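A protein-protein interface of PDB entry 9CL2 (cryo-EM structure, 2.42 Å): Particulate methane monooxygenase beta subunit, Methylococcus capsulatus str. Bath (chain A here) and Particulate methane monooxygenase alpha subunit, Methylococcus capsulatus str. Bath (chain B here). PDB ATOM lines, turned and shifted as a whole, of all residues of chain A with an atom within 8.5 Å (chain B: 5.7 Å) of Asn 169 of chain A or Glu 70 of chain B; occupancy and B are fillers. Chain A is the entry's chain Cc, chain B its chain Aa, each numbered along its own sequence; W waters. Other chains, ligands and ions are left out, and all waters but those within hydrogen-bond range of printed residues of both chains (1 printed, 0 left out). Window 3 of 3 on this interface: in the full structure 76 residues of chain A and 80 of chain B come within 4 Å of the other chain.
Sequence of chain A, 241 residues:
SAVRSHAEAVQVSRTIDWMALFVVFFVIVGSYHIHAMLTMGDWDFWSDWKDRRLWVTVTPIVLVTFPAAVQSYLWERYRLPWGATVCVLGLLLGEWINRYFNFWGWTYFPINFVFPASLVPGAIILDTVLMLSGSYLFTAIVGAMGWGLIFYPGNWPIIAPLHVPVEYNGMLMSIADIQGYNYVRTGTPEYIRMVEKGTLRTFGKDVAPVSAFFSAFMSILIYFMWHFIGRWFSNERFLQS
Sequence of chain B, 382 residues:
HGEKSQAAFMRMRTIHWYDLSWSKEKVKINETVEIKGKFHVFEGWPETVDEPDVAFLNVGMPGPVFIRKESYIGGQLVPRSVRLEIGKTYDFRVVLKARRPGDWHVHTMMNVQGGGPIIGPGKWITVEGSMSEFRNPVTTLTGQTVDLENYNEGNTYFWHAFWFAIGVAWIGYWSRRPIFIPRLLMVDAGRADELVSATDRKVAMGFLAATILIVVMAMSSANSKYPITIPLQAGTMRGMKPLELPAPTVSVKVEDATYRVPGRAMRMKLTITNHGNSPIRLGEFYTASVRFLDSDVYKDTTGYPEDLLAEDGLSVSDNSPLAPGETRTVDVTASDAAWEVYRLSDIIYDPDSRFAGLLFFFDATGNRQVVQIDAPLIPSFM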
ATOM      1  N   VAL A 166      18.882 -15.961  -3.556  1.00  0.00           N
ATOM      2  CA  VAL A 166      18.291 -17.025  -2.755  1.00  0.00           C
ATOM      3  C   VAL A 166      19.412 -17.772  -2.047  1.00  0.00           C
ATOM      4  O   VAL A 166      20.489 -17.978  -2.617  1.00  0.00           O
ATOM      5  CB  VAL A 166      17.454 -17.995  -3.620  1.00  0.00           C
ATOM      6  CG1 VAL A 166      16.837 -19.089  -2.763  1.00  0.00           C
ATOM      7  CG2 VAL A 166      16.370 -17.247  -4.383  1.00  0.00           C
ATOM      8  N   GLU A 167      19.170 -18.161  -0.798  1.00  0.00           N
ATOM      9  CA  GLU A 167      20.106 -19.015  -0.067  1.00  0.00           C
ATOM     10  C   GLU A 167      19.658 -20.456  -0.268  1.00  0.00           C
ATOM     11  O   GLU A 167      18.855 -20.994   0.496  1.00  0.00           O
ATOM     12  CB  GLU A 167      20.161 -18.631   1.406  1.00  0.00           C
ATOM     13  CG  GLU A 167      21.467 -18.999   2.091  1.00  0.00           C
ATOM     14  CD  GLU A 167      21.308 -20.139   3.078  1.00  0.00           C
ATOM     15  OE1 GLU A 167      22.119 -20.220   4.025  1.00  0.00           O
ATOM     16  OE2 GLU A 167      20.375 -20.950   2.909  1.00  0.00           O
ATOM     17  N   TYR A 168      20.180 -21.088  -1.316  1.00  0.00           N
ATOM     18  CA  TYR A 168      19.799 -22.441  -1.697  1.00  0.00           C
ATOM     19  C   TYR A 168      20.812 -23.412  -1.102  1.00  0.00           C
ATOM     20  O   TYR A 168      21.973 -23.447  -1.526  1.00  0.00           O
ATOM     21  CB  TYR A 168      19.736 -22.571  -3.217  1.00  0.00           C
ATOM     22  CG  TYR A 168      19.001 -23.797  -3.708  1.00  0.00           C
ATOM     23  CD1 TYR A 168      17.613 -23.833  -3.741  1.00  0.00           C
ATOM     24  CD2 TYR A 168      19.695 -24.919  -4.142  1.00  0.00           C
ATOM     25  CE1 TYR A 168      16.939 -24.951  -4.191  1.00  0.00           C
ATOM     26  CE2 TYR A 168      19.030 -26.039  -4.594  1.00  0.00           C
ATOM     27  CZ  TYR A 168      17.652 -26.051  -4.617  1.00  0.00           C
ATOM     28  OH  TYR A 168      16.985 -27.167  -5.065  1.00  0.00           O
ATOM     29  N   ASN A 169      20.372 -24.180  -0.101  1.00  0.00           N
ATOM     30  CA  ASN A 169      21.179 -25.235   0.513  1.00  0.00           C
ATOM     31  C   ASN A 169      22.534 -24.717   0.987  1.00  0.00           C
ATOM     32  O   ASN A 169      23.548 -25.416   0.901  1.00  0.00           O
ATOM     33  CB  ASN A 169      21.357 -26.416  -0.443  1.00  0.00           C
ATOM     34  CG  ASN A 169      20.086 -27.226  -0.609  1.00  0.00           C
ATOM     35  OD1 ASN A 169      19.555 -27.353  -1.711  1.00  0.00           O
ATOM     36  ND2 ASN A 169      19.590 -27.777   0.493  1.00  0.00           N
ATOM     37  N   GLY A 170      22.565 -23.484   1.489  1.00  0.00           N
ATOM     38  CA  GLY A 170      23.764 -22.895   2.033  1.00  0.00           C
ATOM     39  C   GLY A 170      24.590 -22.095   1.046  1.00  0.00           C
ATOM     40  O   GLY A 170      25.562 -21.452   1.458  1.00  0.00           O
ATOM     41  N   MET A 171      24.242 -22.119  -0.236  1.00  0.00           N
ATOM     42  CA  MET A 171      24.980 -21.385  -1.254  1.00  0.00           C
ATOM     43  C   MET A 171      24.112 -20.283  -1.844  1.00  0.00           C
ATOM     44  O   MET A 171      22.900 -20.445  -2.004  1.00  0.00           O
ATOM     45  CB  MET A 171      25.460 -22.322  -2.367  1.00  0.00           C
ATOM     46  CG  MET A 171      26.818 -22.951  -2.106  1.00  0.00           C
ATOM     47  SD  MET A 171      27.422 -23.925  -3.497  1.00  0.00           S
ATOM     48  CE  MET A 171      28.267 -22.665  -4.450  1.00  0.00           C
ATOM     49  N   LEU A 172      24.738 -19.153  -2.164  1.00  0.00           N
ATOM     50  CA  LEU A 172      24.015 -18.053  -2.789  1.00  0.00           C
ATOM     51  C   LEU A 172      23.756 -18.393  -4.250  1.00  0.00           C
ATOM     52  O   LEU A 172      24.682 -18.754  -4.984  1.00  0.00           O
ATOM     53  CB  LEU A 172      24.791 -16.745  -2.669  1.00  0.00           C
ATOM     54  CG  LEU A 172      24.045 -15.554  -3.280  1.00  0.00           C
ATOM     55  CD1 LEU A 172      22.859 -15.174  -2.412  1.00  0.00           C
ATOM     56  CD2 LEU A 172      24.962 -14.362  -3.482  1.00  0.00           C
ATOM     57  N   MET A 173      22.499 -18.283  -4.669  1.00  0.00           N
ATOM     58  CA  MET A 173      22.080 -18.652  -6.008  1.00  0.00           C
ATOM     59  C   MET A 173      21.132 -17.589  -6.543  1.00  0.00           C
ATOM     60  O   MET A 173      20.510 -16.840  -5.785  1.00  0.00           O
ATOM     61  CB  MET A 173      21.395 -20.027  -6.016  1.00  0.00           C
ATOM     62  CG  MET A 173      22.301 -21.182  -5.600  1.00  0.00           C
ATOM     63  SD  MET A 173      21.942 -22.739  -6.432  1.00  0.00           S
ATOM     64  CE  MET A 173      22.279 -22.310  -8.135  1.00  0.00           C
ATOM     65  N   ILE A 178      18.833 -21.236 -10.018  1.00  0.00           N
ATOM     66  CA  ILE A 178      18.068 -22.345  -9.456  1.00  0.00           C
ATOM     67  C   ILE A 178      17.202 -22.996 -10.530  1.00  0.00           C
ATOM     68  O   ILE A 178      16.995 -24.214 -10.522  1.00  0.00           O
ATOM     69  CB  ILE A 178      17.229 -21.866  -8.257  1.00  0.00           C
ATOM     70  CG1 ILE A 178      18.143 -21.376  -7.136  1.00  0.00           C
ATOM     71  CG2 ILE A 178      16.339 -22.982  -7.739  1.00  0.00           C
ATOM     72  CD1 ILE A 178      17.398 -20.812  -5.957  1.00  0.00           C
ATOM     73  N   TYR A 181      19.476 -25.216 -12.354  1.00  0.00           N
ATOM     74  CA  TYR A 181      19.878 -26.344 -11.517  1.00  0.00           C
ATOM     75  C   TYR A 181      18.775 -27.394 -11.422  1.00  0.00           C
ATOM     76  O   TYR A 181      19.032 -28.592 -11.589  1.00  0.00           O
ATOM     77  CB  TYR A 181      20.257 -25.834 -10.127  1.00  0.00           C
ATOM     78  CG  TYR A 181      20.911 -26.861  -9.238  1.00  0.00           C
ATOM     79  CD1 TYR A 181      21.994 -27.605  -9.682  1.00  0.00           C
ATOM     80  CD2 TYR A 181      20.449 -27.080  -7.950  1.00  0.00           C
ATOM     81  CE1 TYR A 181      22.595 -28.542  -8.867  1.00  0.00           C
ATOM     82  CE2 TYR A 181      21.041 -28.013  -7.128  1.00  0.00           C
ATOM     83  CZ  TYR A 181      22.114 -28.742  -7.590  1.00  0.00           C
ATOM     84  OH  TYR A 181      22.707 -29.673  -6.771  1.00  0.00           O
ATOM     85  N   ASN A 182      17.543 -26.963 -11.151  1.00  0.00           N
ATOM     86  CA  ASN A 182      16.465 -27.907 -10.877  1.00  0.00           C
ATOM     87  C   ASN A 182      16.042 -28.653 -12.135  1.00  0.00           C
ATOM     88  O   ASN A 182      15.908 -29.882 -12.125  1.00  0.00           O
ATOM     89  CB  ASN A 182      15.272 -27.173 -10.263  1.00  0.00           C
ATOM     90  CG  ASN A 182      15.464 -26.881  -8.790  1.00  0.00           C
ATOM     91  OD1 ASN A 182      16.296 -27.497  -8.125  1.00  0.00           O
ATOM     92  ND2 ASN A 182      14.689 -25.936  -8.271  1.00  0.00           N
ATOM     93  N   ARG B  68      16.138 -31.938 -10.154  1.00  0.00           N
ATOM     94  CA  ARG B  68      17.268 -32.271  -9.292  1.00  0.00           C
ATOM     95  C   ARG B  68      17.236 -31.318  -8.106  1.00  0.00           C
ATOM     96  O   ARG B  68      17.657 -30.163  -8.205  1.00  0.00           O
ATOM     97  CB  ARG B  68      18.579 -32.186 -10.066  1.00  0.00           C
ATOM     98  CG  ARG B  68      19.828 -32.162  -9.206  1.00  0.00           C
ATOM     99  CD  ARG B  68      20.945 -31.406  -9.894  1.00  0.00           C
ATOM    100  NE  ARG B  68      21.448 -32.106 -11.069  1.00  0.00           N
ATOM    101  CZ  ARG B  68      21.525 -31.574 -12.282  1.00  0.00           C
ATOM    102  NH1 ARG B  68      21.134 -30.333 -12.517  1.00  0.00           N
ATOM    103  NH2 ARG B  68      22.004 -32.307 -13.283  1.00  0.00           N
ATOM    104  N   LYS B  69      16.700 -31.798  -6.981  1.00  0.00           N
ATOM    105  CA  LYS B  69      16.623 -30.958  -5.792  1.00  0.00           C
ATOM    106  C   LYS B  69      18.011 -30.611  -5.275  1.00  0.00           C
ATOM    107  O   LYS B  69      18.280 -29.452  -4.936  1.00  0.00           O
ATOM    108  CB  LYS B  69      15.799 -31.650  -4.708  1.00  0.00           C
ATOM    109  CG  LYS B  69      14.317 -31.324  -4.756  1.00  0.00           C
ATOM    110  CD  LYS B  69      14.088 -29.845  -5.020  1.00  0.00           C
ATOM    111  CE  LYS B  69      13.805 -29.090  -3.733  1.00  0.00           C
ATOM    112  NZ  LYS B  69      13.973 -27.621  -3.906  1.00  0.00           N
ATOM    113  N   GLU B  70      18.910 -31.592  -5.215  1.00  0.00           N
ATOM    114  CA  GLU B  70      20.269 -31.295  -4.780  1.00  0.00           C
ATOM    115  C   GLU B  70      21.217 -32.392  -5.238  1.00  0.00           C
ATOM    116  O   GLU B  70      20.801 -33.504  -5.570  1.00  0.00           O
ATOM    117  CB  GLU B  70      20.347 -31.118  -3.260  1.00  0.00           C
ATOM    118  CG  GLU B  70      19.698 -32.229  -2.467  1.00  0.00           C
ATOM    119  CD  GLU B  70      18.967 -31.718  -1.243  1.00  0.00           C
ATOM    120  OE1 GLU B  70      18.197 -30.743  -1.375  1.00  0.00           O
ATOM    121  OE2 GLU B  70      19.163 -32.288  -0.150  1.00  0.00           O
ATOM    122  N   SER B  71      22.505 -32.056  -5.243  1.00  0.00           N
ATOM    123  CA  SER B  71      23.565 -32.988  -5.601  1.00  0.00           C
ATOM    124  C   SER B  71      24.788 -32.690  -4.748  1.00  0.00           C
ATOM    125  O   SER B  71      25.170 -31.527  -4.591  1.00  0.00           O
ATOM    126  CB  SER B  71      23.913 -32.891  -7.091  1.00  0.00           C
ATOM    127  OG  SER B  71      24.348 -31.586  -7.429  1.00  0.00           O
ATOM    128  N   TYR B  72      25.392 -33.740  -4.198  1.00  0.00           N
ATOM    129  CA  TYR B  72      26.537 -33.633  -3.308  1.00  0.00           C
ATOM    130  C   TYR B  72      27.653 -34.533  -3.811  1.00  0.00           C
ATOM    131  O   TYR B  72      27.413 -35.702  -4.132  1.00  0.00           O
ATOM    132  CB  TYR B  72      26.169 -34.032  -1.875  1.00  0.00           C
ATOM    133  CG  TYR B  72      25.062 -33.215  -1.256  1.00  0.00           C
ATOM    134  CD1 TYR B  72      25.338 -32.042  -0.568  1.00  0.00           C
ATOM    135  CD2 TYR B  72      23.739 -33.624  -1.348  1.00  0.00           C
ATOM    136  CE1 TYR B  72      24.328 -31.297   0.004  1.00  0.00           C
ATOM    137  CE2 TYR B  72      22.722 -32.885  -0.780  1.00  0.00           C
ATOM    138  CZ  TYR B  72      23.022 -31.722  -0.105  1.00  0.00           C
ATOM    139  OH  TYR B  72      22.012 -30.982   0.464  1.00  0.00           O
ATOM    140  N   LEU B  77      27.615 -29.717  -1.531  1.00  0.00           N
ATOM    141  CA  LEU B  77      26.697 -29.402  -2.619  1.00  0.00           C
ATOM    142  C   LEU B  77      27.467 -28.895  -3.831  1.00  0.00           C
ATOM    143  O   LEU B  77      28.393 -28.089  -3.709  1.00  0.00           O
ATOM    144  CB  LEU B  77      25.678 -28.357  -2.166  1.00  0.00           C
ATOM    145  CG  LEU B  77      24.574 -28.016  -3.168  1.00  0.00           C
ATOM    146  CD1 LEU B  77      23.401 -28.974  -3.021  1.00  0.00           C
ATOM    147  CD2 LEU B  77      24.121 -26.574  -3.004  1.00  0.00           C
ATOM    148  N   ARG B  93      25.860 -38.178  -4.017  1.00  0.00           N
ATOM    149  CA  ARG B  93      24.459 -38.285  -3.641  1.00  0.00           C
ATOM    150  C   ARG B  93      23.654 -37.325  -4.502  1.00  0.00           C
ATOM    151  O   ARG B  93      24.096 -36.207  -4.768  1.00  0.00           O
ATOM    152  CB  ARG B  93      24.249 -37.964  -2.154  1.00  0.00           C
ATOM    153  CG  ARG B  93      22.838 -38.222  -1.654  1.00  0.00           C
ATOM    154  CD  ARG B  93      22.762 -38.150  -0.138  1.00  0.00           C
ATOM    155  NE  ARG B  93      21.833 -37.123   0.316  1.00  0.00           N
ATOM    156  CZ  ARG B  93      22.191 -35.997   0.916  1.00  0.00           C
ATOM    157  NH1 ARG B  93      23.460 -35.717   1.158  1.00  0.00           N
ATOM    158  NH2 ARG B  93      21.252 -35.131   1.283  1.00  0.00           N
ATOM    159  N   VAL B  94      22.486 -37.767  -4.957  1.00  0.00           N
ATOM    160  CA  VAL B  94      21.603 -36.928  -5.759  1.00  0.00           C
ATOM    161  C   VAL B  94      20.184 -37.105  -5.241  1.00  0.00           C
ATOM    162  O   VAL B  94      19.679 -38.231  -5.184  1.00  0.00           O
ATOM    163  CB  VAL B  94      21.672 -37.270  -7.258  1.00  0.00           C
ATOM    164  CG1 VAL B  94      20.565 -36.559  -8.014  1.00  0.00           C
ATOM    165  CG2 VAL B  94      23.030 -36.895  -7.831  1.00  0.00           C
ATOM    166  N   VAL B  95      19.539 -36.004  -4.869  1.00  0.00           N
ATOM    167  CA  VAL B  95      18.149 -36.012  -4.433  1.00  0.00           C
ATOM    168  C   VAL B  95      17.324 -35.349  -5.525  1.00  0.00           C
ATOM    169  O   VAL B  95      17.545 -34.172  -5.851  1.00  0.00           O
ATOM    170  CB  VAL B  95      17.967 -35.295  -3.088  1.00  0.00           C
ATOM    171  CG1 VAL B  95      16.544 -35.471  -2.583  1.00  0.00           C
ATOM    172  CG2 VAL B  95      18.970 -35.816  -2.072  1.00  0.00           C
ATOM    173  N   LEU B  96      16.377 -36.106  -6.081  1.00  0.00           N
ATOM    174  CA  LEU B  96      15.511 -35.666  -7.163  1.00  0.00           C
ATOM    175  C   LEU B  96      14.067 -35.641  -6.681  1.00  0.00           C
ATOM    176  O   LEU B  96      13.688 -36.393  -5.782  1.00  0.00           O
ATOM    177  CB  LEU B  96      15.620 -36.594  -8.382  1.00  0.00           C
ATOM    178  CG  LEU B  96      17.004 -36.913  -8.943  1.00  0.00           C
ATOM    179  CD1 LEU B  96      16.978 -38.238  -9.682  1.00  0.00           C
ATOM    180  CD2 LEU B  96      17.470 -35.806  -9.866  1.00  0.00           C
HETATM  181  O   HOH W   1      13.881 -25.962  -5.815  1.00  0.00           O
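O of Tyr 181 of chain A lies within hydrogen-bond range of NH1 of Arg 68 of chain B (2.9 Å). The backbone NH of Arg 68 of chain B sits at hydrogen-bond distance from the backbone carbonyl oxygen of Asn 182 of chain A, 2.9 Å away. The side-chain hydroxyl of Tyr 181 of chain A lies within hydrogen-bond range of the side-chain hydroxyl of Ser 71 of chain B, at 2.6 Å. OH of Tyr 168 of chain A is in hydrogen-bond range of O of Lys 69 of chain B (2.6 Å).
OE2 of Glu 70 of chain B is in salt-bridge range of NH2 of Arg 93 of chain B. OH of Tyr 168 of chain A sits at hydrogen-bond distance from OD1 of Asn 182 of chain A (3.2 Å). OE2 of Glu 70 of chain B sits at hydrogen-bond distance from OH of Tyr 72 of chain B. O of Val 95 of chain B sits at hydrogen-bond distance from N of Lys 69 of chain B (2.8 Å). The backbone carbonyl oxygen (O) of Glu 70 of chain B lies within hydrogen-bond range of the backbone NH (N) of Val 95 of chain B.
OD1 of Asn 169 of chain A touches OE1 of Glu 70 of chain B, at 3.7 Å. Asn 169 of chain A touches Leu 77 of chain B. Lys 69 of chain B touches Tyr 181 of chain A. Tyr 181 of chain A touches Glu 70 of chain B (OH to C, 3.5 Å). Tyr 181 of chain A touches Leu 77 of chain B (OH to CD1, 3.9 Å).
Printed residues of chain B within 4 Å of Asn 169 of chain A: Glu 70 (3.7 Å) and Leu 77 (3.8 Å). Glu 70 of chain B touches just these residues of chain A: Asn 169 (3.7 Å) and Tyr 181 (3.5 Å). Ser 71 of chain B touches just one residue of chain A: Tyr 181. Of the printed residues of chain A, Lys 69 of chain B touches Tyr 168 and Tyr 181. Printed residues of chain B within 4 Å of Tyr 168 of chain A: Lys 69. Of the printed residues of chain A, Leu 77 of chain B touches Asn 169 (3.8 Å) and Tyr 181 (3.9 Å). Of the printed residues of chain B, Asn 182 of chain A touches Arg 68. Of the printed residues of chain B, Tyr 181 of chain A touches Arg 68, Lys 69, Glu 70, Ser 71 and Leu 77. Leu 172 of chain A touches none of the printed residues of chain B. The nearest printed residue of chain B that does not touch Asn 169 of chain A is Tyr 72 of chain B (4.02 Å). The nearest residue of chain A that does not touch Glu 70 of chain B is Tyr 168 of chain A (4.8 Å). The nearest printed residue of chain B that does not touch Asn 182 of chain A is Lys 69 of chain B (4.2 Å).
Water W1 lies within hydrogen-bond range of the side-chain amino group (NZ) of Lys 69 of chain B (2.5 Å), the side-chain amide nitrogen (ND2) of Asn 182 of chain A (2.6 Å) and the side-chain hydroxyl (OH) of Tyr 168 of chain A (3.4 Å).
Hydrophobic or aromatic side chains of chain A that line the printed part of chain B: Tyr 168 and Tyr 181. Among the printed residues, 9 pairs touch across the chains. Among the printed residues, no Asp or Glu carboxylate lies within 4 Å of a Lys or Arg side-chain nitrogen of the other chain.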
